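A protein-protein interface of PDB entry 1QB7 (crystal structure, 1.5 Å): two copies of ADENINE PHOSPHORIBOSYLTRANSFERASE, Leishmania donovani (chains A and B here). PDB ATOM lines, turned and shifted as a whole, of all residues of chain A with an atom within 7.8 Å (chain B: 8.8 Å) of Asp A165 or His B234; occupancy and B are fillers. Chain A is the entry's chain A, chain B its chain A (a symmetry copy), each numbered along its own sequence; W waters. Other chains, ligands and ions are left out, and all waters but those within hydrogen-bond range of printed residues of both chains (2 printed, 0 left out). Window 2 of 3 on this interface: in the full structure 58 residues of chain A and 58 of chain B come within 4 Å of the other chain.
The side-chain carboxylate (OE1) of Glu B233 lies within hydrogen-bond range of the side-chain hydroxyl (OH) of Tyr A132 (2.8 Å).
Water W2 bridges O of Pro B235 (2.6 Å) and OD2 of Asp A165 (2.9 Å). Water W1 lies within hydrogen-bond range of O of Glu A162 (2.8 Å) and NE2 of His B234 (3.1 Å).
CA of Cys B227 touches CG2 of Ile A111, at 3.9 Å. Val B230 touches Ile A111 (CG2 to CG2, 3.8 Å). Val B230 touches Tyr A132. CB of Cys B227 touches CB of Ala A163, at 3.6 Å. Ala A163 touches Val B230. CG of Leu B231 touches CA of Ala A163, at 3.97 Å. O of Ala A163 touches CE1 of His B234, 3.0 Å away. Asp A165 touches His B234.
No position is printed for both chains. Of the 9 pairs that touch across the chains among the printed residues, none has its exchanged pair printed and touching as well.
Printed residues of chain B within 4 Å of Ile A111: Cys B227 and Val B230. Gln A159 touches none of the printed residues of chain B. Of chain B, only His B234 comes within 4 Å of Asp A165. No residue of chain B comes within 4 Å of Ala A166. Of the printed residues of chain A, Cys B227 touches Ile A111 (3.9 Å) and Ala A163 (3.6 Å). Of the printed residues of chain A, Val B230 touches Ile A111 (3.8 Å), Tyr A132 (3.7 Å) and Ala A163 (3.4 Å). Of the printed residues of chain A, Leu B231 touches Ala A163. Printed residues of chain A within 4 Å of Glu B233: Tyr A132. Of chain A, only Ala A163 and Asp A165 come within 4 Å of His B234. The nearest residue of chain B that does not touch Asp A165 is Pro B235 (4.8 Å). The nearest printed residue of chain A that does not touch His B234 is Glu A162 (4.2 Å).
Of the 10 printed residues of chain B, 5 touch a printed residue of chain A. Hydrophobic or aromatic side chains of chain B that line the printed part of chain A: Val B230, Leu B231 and His B234. Printed residues of chain A that touch a printed residue of chain B: Ile A111, Tyr A132, Ala A163 and Asp A165. Among the printed residues, 9 pairs touch across the chains. Among the printed residues, no Asp or Glu carboxylate lies within 4 Å of a Lys or Arg side-chain nitrogen of the other chain.
The backbone carbonyl oxygen (O) of Leu B231 lies within hydrogen-bond range of a ring nitrogen (ND1) of His B236 (3.1 Å). The backbone carbonyl oxygen (O) of Asp A165 sits at hydrogen-bond distance from the backbone NH (N) of Gly A138, at 3.4 Å. The backbone carbonyl oxygen (O) of Val B230 lies within hydrogen-bond range of a ring nitrogen (ND1) of His B234 (3.4 Å). The backbone carbonyl oxygen (O) of His B234 lies within hydrogen-bond range of a ring nitrogen (ND1) of His B236 (3.0 Å).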
ATOM      1  N   ILE A 111     -20.001  28.250   9.876  1.00  0.00           N
ATOM      2  CA  ILE A 111     -21.426  28.087  10.139  1.00  0.00           C
ATOM      3  C   ILE A 111     -21.914  29.532  10.200  1.00  0.00           C
ATOM      4  O   ILE A 111     -21.338  30.332  10.933  1.00  0.00           O
ATOM      5  CB  ILE A 111     -21.712  27.441  11.524  1.00  0.00           C
ATOM      6  CG1 ILE A 111     -20.995  26.095  11.655  1.00  0.00           C
ATOM      7  CG2 ILE A 111     -23.230  27.270  11.719  1.00  0.00           C
ATOM      8  CD1 ILE A 111     -21.170  25.437  13.010  1.00  0.00           C
ATOM      9  N   TYR A 132     -16.762  25.932  11.771  1.00  0.00           N
ATOM     10  CA  TYR A 132     -17.445  24.684  12.071  1.00  0.00           C
ATOM     11  C   TYR A 132     -16.541  23.831  12.956  1.00  0.00           C
ATOM     12  O   TYR A 132     -15.402  23.561  12.596  1.00  0.00           O
ATOM     13  CB  TYR A 132     -17.724  23.947  10.758  1.00  0.00           C
ATOM     14  CG  TYR A 132     -18.480  22.654  10.906  1.00  0.00           C
ATOM     15  CD1 TYR A 132     -17.808  21.453  11.130  1.00  0.00           C
ATOM     16  CD2 TYR A 132     -19.868  22.625  10.799  1.00  0.00           C
ATOM     17  CE1 TYR A 132     -18.503  20.253  11.243  1.00  0.00           C
ATOM     18  CE2 TYR A 132     -20.572  21.434  10.907  1.00  0.00           C
ATOM     19  CZ  TYR A 132     -19.888  20.251  11.127  1.00  0.00           C
ATOM     20  OH  TYR A 132     -20.587  19.065  11.210  1.00  0.00           O
ATOM     21  N   ILE A 135     -16.649  24.891  18.411  1.00  0.00           N
ATOM     22  CA  ILE A 135     -17.381  24.580  19.629  1.00  0.00           C
ATOM     23  C   ILE A 135     -18.080  23.266  19.344  1.00  0.00           C
ATOM     24  O   ILE A 135     -18.732  23.108  18.313  1.00  0.00           O
ATOM     25  CB  ILE A 135     -18.436  25.660  20.020  1.00  0.00           C
ATOM     26  CG1 ILE A 135     -17.802  27.048  20.078  1.00  0.00           C
ATOM     27  CG2 ILE A 135     -19.132  25.289  21.294  1.00  0.00           C
ATOM     28  CD1 ILE A 135     -18.816  28.167  20.142  1.00  0.00           C
ATOM     29  N   GLY A 136     -17.898  22.298  20.228  1.00  0.00           N
ATOM     30  CA  GLY A 136     -18.516  21.007  20.008  1.00  0.00           C
ATOM     31  C   GLY A 136     -19.671  20.711  20.933  1.00  0.00           C
ATOM     32  O   GLY A 136     -20.052  21.539  21.762  1.00  0.00           O
ATOM     33  N   LYS A 137     -20.238  19.524  20.758  1.00  0.00           N
ATOM     34  CA  LYS A 137     -21.345  19.053  21.575  1.00  0.00           C
ATOM     35  C   LYS A 137     -20.891  19.036  23.026  1.00  0.00           C
ATOM     36  O   LYS A 137     -19.763  18.636  23.329  1.00  0.00           O
ATOM     37  CB  LYS A 137     -21.738  17.640  21.138  1.00  0.00           C
ATOM     38  CG  LYS A 137     -22.833  16.989  21.962  1.00  0.00           C
ATOM     39  CD  LYS A 137     -23.183  15.635  21.368  1.00  0.00           C
ATOM     40  CE  LYS A 137     -24.290  14.944  22.142  1.00  0.00           C
ATOM     41  NZ  LYS A 137     -24.547  13.579  21.585  1.00  0.00           N
ATOM     42  N   GLY A 138     -21.750  19.524  23.912  1.00  0.00           N
ATOM     43  CA  GLY A 138     -21.405  19.549  25.317  1.00  0.00           C
ATOM     44  C   GLY A 138     -20.697  20.804  25.796  1.00  0.00           C
ATOM     45  O   GLY A 138     -20.563  20.999  27.004  1.00  0.00           O
ATOM     46  N   SER A 139     -20.242  21.649  24.870  1.00  0.00           N
ATOM     47  CA  SER A 139     -19.554  22.891  25.237  1.00  0.00           C
ATOM     48  C   SER A 139     -20.492  23.859  25.946  1.00  0.00           C
ATOM     49  O   SER A 139     -21.684  23.918  25.650  1.00  0.00           O
ATOM     50  CB  SER A 139     -18.985  23.592  24.003  1.00  0.00           C
ATOM     51  OG  SER A 139     -18.061  22.779  23.302  1.00  0.00           O
ATOM     52  N   ARG A 140     -19.944  24.588  26.909  1.00  0.00           N
ATOM     53  CA  ARG A 140     -20.693  25.583  27.663  1.00  0.00           C
ATOM     54  C   ARG A 140     -19.977  26.888  27.342  1.00  0.00           C
ATOM     55  O   ARG A 140     -18.878  27.157  27.829  1.00  0.00           O
ATOM     56  CB  ARG A 140     -20.674  25.235  29.150  1.00  0.00           C
ATOM     57  CG  ARG A 140     -21.403  23.922  29.452  1.00  0.00           C
ATOM     58  CD  ARG A 140     -21.333  23.534  30.924  1.00  0.00           C
ATOM     59  NE  ARG A 140     -19.962  23.275  31.366  1.00  0.00           N
ATOM     60  CZ  ARG A 140     -19.302  22.130  31.178  1.00  0.00           C
ATOM     61  NH1 ARG A 140     -19.883  21.113  30.552  1.00  0.00           N
ATOM     62  NH2 ARG A 140     -18.058  22.001  31.625  1.00  0.00           N
ATOM     63  N   GLN A 159     -27.711  31.455  18.119  1.00  0.00           N
ATOM     64  CA  GLN A 159     -27.981  30.537  17.018  1.00  0.00           C
ATOM     65  C   GLN A 159     -26.775  29.656  16.711  1.00  0.00           C
ATOM     66  O   GLN A 159     -26.909  28.448  16.536  1.00  0.00           O
ATOM     67  CB  GLN A 159     -28.378  31.316  15.762  1.00  0.00           C
ATOM     68  CG  GLN A 159     -29.700  32.056  15.881  1.00  0.00           C
ATOM     69  CD  GLN A 159     -30.005  32.916  14.669  1.00  0.00           C
ATOM     70  OE1 GLN A 159     -29.101  33.342  13.946  1.00  0.00           O
ATOM     71  NE2 GLN A 159     -31.286  33.195  14.452  1.00  0.00           N
ATOM     72  N   LEU A 160     -25.599  30.276  16.647  1.00  0.00           N
ATOM     73  CA  LEU A 160     -24.366  29.562  16.342  1.00  0.00           C
ATOM     74  C   LEU A 160     -24.014  28.524  17.403  1.00  0.00           C
ATOM     75  O   LEU A 160     -23.588  27.417  17.073  1.00  0.00           O
ATOM     76  CB  LEU A 160     -23.218  30.556  16.125  1.00  0.00           C
ATOM     77  CG  LEU A 160     -23.349  31.436  14.874  1.00  0.00           C
ATOM     78  CD1 LEU A 160     -22.346  32.575  14.918  1.00  0.00           C
ATOM     79  CD2 LEU A 160     -23.185  30.597  13.605  1.00  0.00           C
ATOM     80  N   VAL A 161     -24.217  28.869  18.673  1.00  0.00           N
ATOM     81  CA  VAL A 161     -23.937  27.943  19.769  1.00  0.00           C
ATOM     82  C   VAL A 161     -24.938  26.776  19.749  1.00  0.00           C
ATOM     83  O   VAL A 161     -24.548  25.620  19.887  1.00  0.00           O
ATOM     84  CB  VAL A 161     -23.952  28.661  21.146  1.00  0.00           C
ATOM     85  CG1 VAL A 161     -23.778  27.652  22.271  1.00  0.00           C
ATOM     86  CG2 VAL A 161     -22.841  29.700  21.213  1.00  0.00           C
ATOM     87  N   GLU A 162     -26.219  27.075  19.538  1.00  0.00           N
ATOM     88  CA  GLU A 162     -27.244  26.029  19.477  1.00  0.00           C
ATOM     89  C   GLU A 162     -26.970  25.077  18.313  1.00  0.00           C
ATOM     90  O   GLU A 162     -27.025  23.863  18.479  1.00  0.00           O
ATOM     91  CB  GLU A 162     -28.658  26.621  19.333  1.00  0.00           C
ATOM     92  CG  GLU A 162     -29.739  25.638  18.907  1.00  0.00           C
ATOM     93  CD  GLU A 162     -31.092  26.297  18.728  1.00  0.00           C
ATOM     94  OE1 GLU A 162     -31.150  27.439  18.216  1.00  0.00           O
ATOM     95  OE2 GLU A 162     -32.101  25.665  19.100  1.00  0.00           O
ATOM     96  N   ALA A 163     -26.678  25.634  17.139  1.00  0.00           N
ATOM     97  CA  ALA A 163     -26.399  24.832  15.952  1.00  0.00           C
ATOM     98  C   ALA A 163     -25.183  23.930  16.157  1.00  0.00           C
ATOM     99  O   ALA A 163     -25.066  22.876  15.526  1.00  0.00           O
ATOM    100  CB  ALA A 163     -26.193  25.733  14.749  1.00  0.00           C
ATOM    101  N   SER A 164     -24.279  24.353  17.038  1.00  0.00           N
ATOM    102  CA  SER A 164     -23.073  23.589  17.350  1.00  0.00           C
ATOM    103  C   SER A 164     -23.351  22.480  18.360  1.00  0.00           C
ATOM    104  O   SER A 164     -22.439  21.752  18.762  1.00  0.00           O
ATOM    105  CB  SER A 164     -22.001  24.518  17.906  1.00  0.00           C
ATOM    106  OG  SER A 164     -21.569  25.419  16.913  1.00  0.00           O
ATOM    107  N   ASP A 165     -24.613  22.367  18.770  1.00  0.00           N
ATOM    108  CA  ASP A 165     -25.048  21.363  19.737  1.00  0.00           C
ATOM    109  C   ASP A 165     -24.433  21.659  21.112  1.00  0.00           C
ATOM    110  O   ASP A 165     -24.133  20.750  21.888  1.00  0.00           O
ATOM    111  CB  ASP A 165     -24.666  19.952  19.248  1.00  0.00           C
ATOM    112  CG  ASP A 165     -25.575  18.858  19.803  1.00  0.00           C
ATOM    113  OD1 ASP A 165     -26.485  19.162  20.604  1.00  0.00           O
ATOM    114  OD2 ASP A 165     -25.382  17.683  19.419  1.00  0.00           O
ATOM    115  N   ALA A 166     -24.256  22.946  21.402  1.00  0.00           N
ATOM    116  CA  ALA A 166     -23.681  23.400  22.668  1.00  0.00           C
ATOM    117  C   ALA A 166     -24.693  24.279  23.398  1.00  0.00           C
ATOM    118  O   ALA A 166     -25.759  24.582  22.866  1.00  0.00           O
ATOM    119  CB  ALA A 166     -22.397  24.189  22.406  1.00  0.00           C
ATOM    120  N   VAL A 167     -24.363  24.677  24.624  1.00  0.00           N
ATOM    121  CA  VAL A 167     -25.253  25.539  25.399  1.00  0.00           C
ATOM    122  C   VAL A 167     -24.577  26.857  25.760  1.00  0.00           C
ATOM    123  O   VAL A 167     -23.353  26.930  25.923  1.00  0.00           O
ATOM    124  CB  VAL A 167     -25.783  24.851  26.705  1.00  0.00           C
ATOM    125  CG1 VAL A 167     -26.644  23.641  26.365  1.00  0.00           C
ATOM    126  CG2 VAL A 167     -24.636  24.440  27.603  1.00  0.00           C
ATOM    127  N   CYS B 227     -26.870  27.696  10.003  1.00  0.00           N
ATOM    128  CA  CYS B 227     -27.123  27.010  11.267  1.00  0.00           C
ATOM    129  C   CYS B 227     -28.161  25.916  11.065  1.00  0.00           C
ATOM    130  O   CYS B 227     -28.022  24.829  11.608  1.00  0.00           O
ATOM    131  CB  CYS B 227     -27.616  27.967  12.357  1.00  0.00           C
ATOM    132  SG  CYS B 227     -28.317  29.524  11.817  1.00  0.00           S
ATOM    133  N   GLY B 228     -29.197  26.219  10.284  1.00  0.00           N
ATOM    134  CA  GLY B 228     -30.241  25.249  10.005  1.00  0.00           C
ATOM    135  C   GLY B 228     -29.680  23.984   9.379  1.00  0.00           C
ATOM    136  O   GLY B 228     -30.099  22.876   9.713  1.00  0.00           O
ATOM    137  N   ASP B 229     -28.730  24.140   8.463  1.00  0.00           N
ATOM    138  CA  ASP B 229     -28.108  22.994   7.818  1.00  0.00           C
ATOM    139  C   ASP B 229     -27.325  22.177   8.844  1.00  0.00           C
ATOM    140  O   ASP B 229     -27.458  20.960   8.888  1.00  0.00           O
ATOM    141  CB  ASP B 229     -27.182  23.442   6.679  1.00  0.00           C
ATOM    142  CG  ASP B 229     -27.950  23.936   5.444  1.00  0.00           C
ATOM    143  OD1 ASP B 229     -29.184  23.751   5.372  1.00  0.00           O
ATOM    144  OD2 ASP B 229     -27.317  24.514   4.532  1.00  0.00           O
ATOM    145  N   VAL B 230     -26.554  22.848   9.700  1.00  0.00           N
ATOM    146  CA  VAL B 230     -25.766  22.152  10.718  1.00  0.00           C
ATOM    147  C   VAL B 230     -26.672  21.469  11.751  1.00  0.00           C
ATOM    148  O   VAL B 230     -26.379  20.359  12.200  1.00  0.00           O
ATOM    149  CB  VAL B 230     -24.754  23.105  11.415  1.00  0.00           C
ATOM    150  CG1 VAL B 230     -23.876  22.328  12.385  1.00  0.00           C
ATOM    151  CG2 VAL B 230     -23.872  23.789  10.377  1.00  0.00           C
ATOM    152  N   LEU B 231     -27.785  22.117  12.100  1.00  0.00           N
ATOM    153  CA  LEU B 231     -28.740  21.558  13.065  1.00  0.00           C
ATOM    154  C   LEU B 231     -29.308  20.224  12.582  1.00  0.00           C
ATOM    155  O   LEU B 231     -29.530  19.306  13.370  1.00  0.00           O
ATOM    156  CB  LEU B 231     -29.898  22.532  13.303  1.00  0.00           C
ATOM    157  CG  LEU B 231     -29.838  23.529  14.459  1.00  0.00           C
ATOM    158  CD1 LEU B 231     -31.043  24.443  14.376  1.00  0.00           C
ATOM    159  CD2 LEU B 231     -29.822  22.804  15.800  1.00  0.00           C
ATOM    160  N   ALA B 232     -29.545  20.127  11.280  1.00  0.00           N
ATOM    161  CA  ALA B 232     -30.089  18.918  10.682  1.00  0.00           C
ATOM    162  C   ALA B 232     -29.139  17.727  10.786  1.00  0.00           C
ATOM    163  O   ALA B 232     -29.559  16.576  10.645  1.00  0.00           O
ATOM    164  CB  ALA B 232     -30.431  19.185   9.221  1.00  0.00           C
ATOM    165  N   GLU B 233     -27.864  18.005  11.040  1.00  0.00           N
ATOM    166  CA  GLU B 233     -26.844  16.960  11.132  1.00  0.00           C
ATOM    167  C   GLU B 233     -26.805  16.194  12.454  1.00  0.00           C
ATOM    168  O   GLU B 233     -26.089  15.200  12.575  1.00  0.00           O
ATOM    169  CB  GLU B 233     -25.464  17.552  10.846  1.00  0.00           C
ATOM    170  CG  GLU B 233     -25.338  18.226   9.487  1.00  0.00           C
ATOM    171  CD  GLU B 233     -24.010  18.951   9.296  1.00  0.00           C
ATOM    172  OE1 GLU B 233     -23.137  18.879  10.195  1.00  0.00           O
ATOM    173  OE2 GLU B 233     -23.844  19.599   8.238  1.00  0.00           O
ATOM    174  N   HIS B 234     -27.557  16.663  13.446  1.00  0.00           N
ATOM    175  CA  HIS B 234     -27.587  16.002  14.748  1.00  0.00           C
ATOM    176  C   HIS B 234     -28.984  16.053  15.366  1.00  0.00           C
ATOM    177  O   HIS B 234     -29.795  16.908  15.012  1.00  0.00           O
ATOM    178  CB  HIS B 234     -26.547  16.628  15.702  1.00  0.00           C
ATOM    179  CG  HIS B 234     -26.787  18.077  16.017  1.00  0.00           C
ATOM    180  ND1 HIS B 234     -26.123  19.100  15.371  1.00  0.00           N
ATOM    181  CD2 HIS B 234     -27.609  18.672  16.915  1.00  0.00           C
ATOM    182  CE1 HIS B 234     -26.526  20.260  15.858  1.00  0.00           C
ATOM    183  NE2 HIS B 234     -27.428  20.029  16.797  1.00  0.00           N
ATOM    184  N   PRO B 235     -29.299  15.098  16.262  1.00  0.00           N
ATOM    185  CA  PRO B 235     -30.612  15.058  16.918  1.00  0.00           C
ATOM    186  C   PRO B 235     -30.817  16.263  17.831  1.00  0.00           C
ATOM    187  O   PRO B 235     -30.024  16.514  18.736  1.00  0.00           O
ATOM    188  CB  PRO B 235     -30.553  13.758  17.725  1.00  0.00           C
ATOM    189  CG  PRO B 235     -29.608  12.909  16.935  1.00  0.00           C
ATOM    190  CD  PRO B 235     -28.520  13.892  16.593  1.00  0.00           C
ATOM    191  N   HIS B 236     -31.881  17.016  17.575  1.00  0.00           N
ATOM    192  CA  HIS B 236     -32.194  18.192  18.379  1.00  0.00           C
ATOM    193  C   HIS B 236     -33.703  18.373  18.505  1.00  0.00           C
ATOM    194  O   HIS B 236     -34.120  19.156  19.387  1.00  0.00           O
ATOM    195  CB  HIS B 236     -31.560  19.447  17.768  1.00  0.00           C
ATOM    196  CG  HIS B 236     -32.109  19.815  16.423  1.00  0.00           C
ATOM    197  ND1 HIS B 236     -31.908  19.042  15.299  1.00  0.00           N
ATOM    198  CD2 HIS B 236     -32.841  20.880  16.021  1.00  0.00           C
ATOM    199  CE1 HIS B 236     -32.493  19.618  14.263  1.00  0.00           C
ATOM    200  NE2 HIS B 236     -33.064  20.735  14.674  1.00  0.00           N
ATOM    201  OXT HIS B 236     -34.447  17.728  17.727  1.00  0.00           O
HETATM  202  O   HOH W   1     -28.826  21.733  18.907  1.00  0.00           O
HETATM  203  O   HOH W   2     -27.767  16.194  20.024  1.00  0.00           O
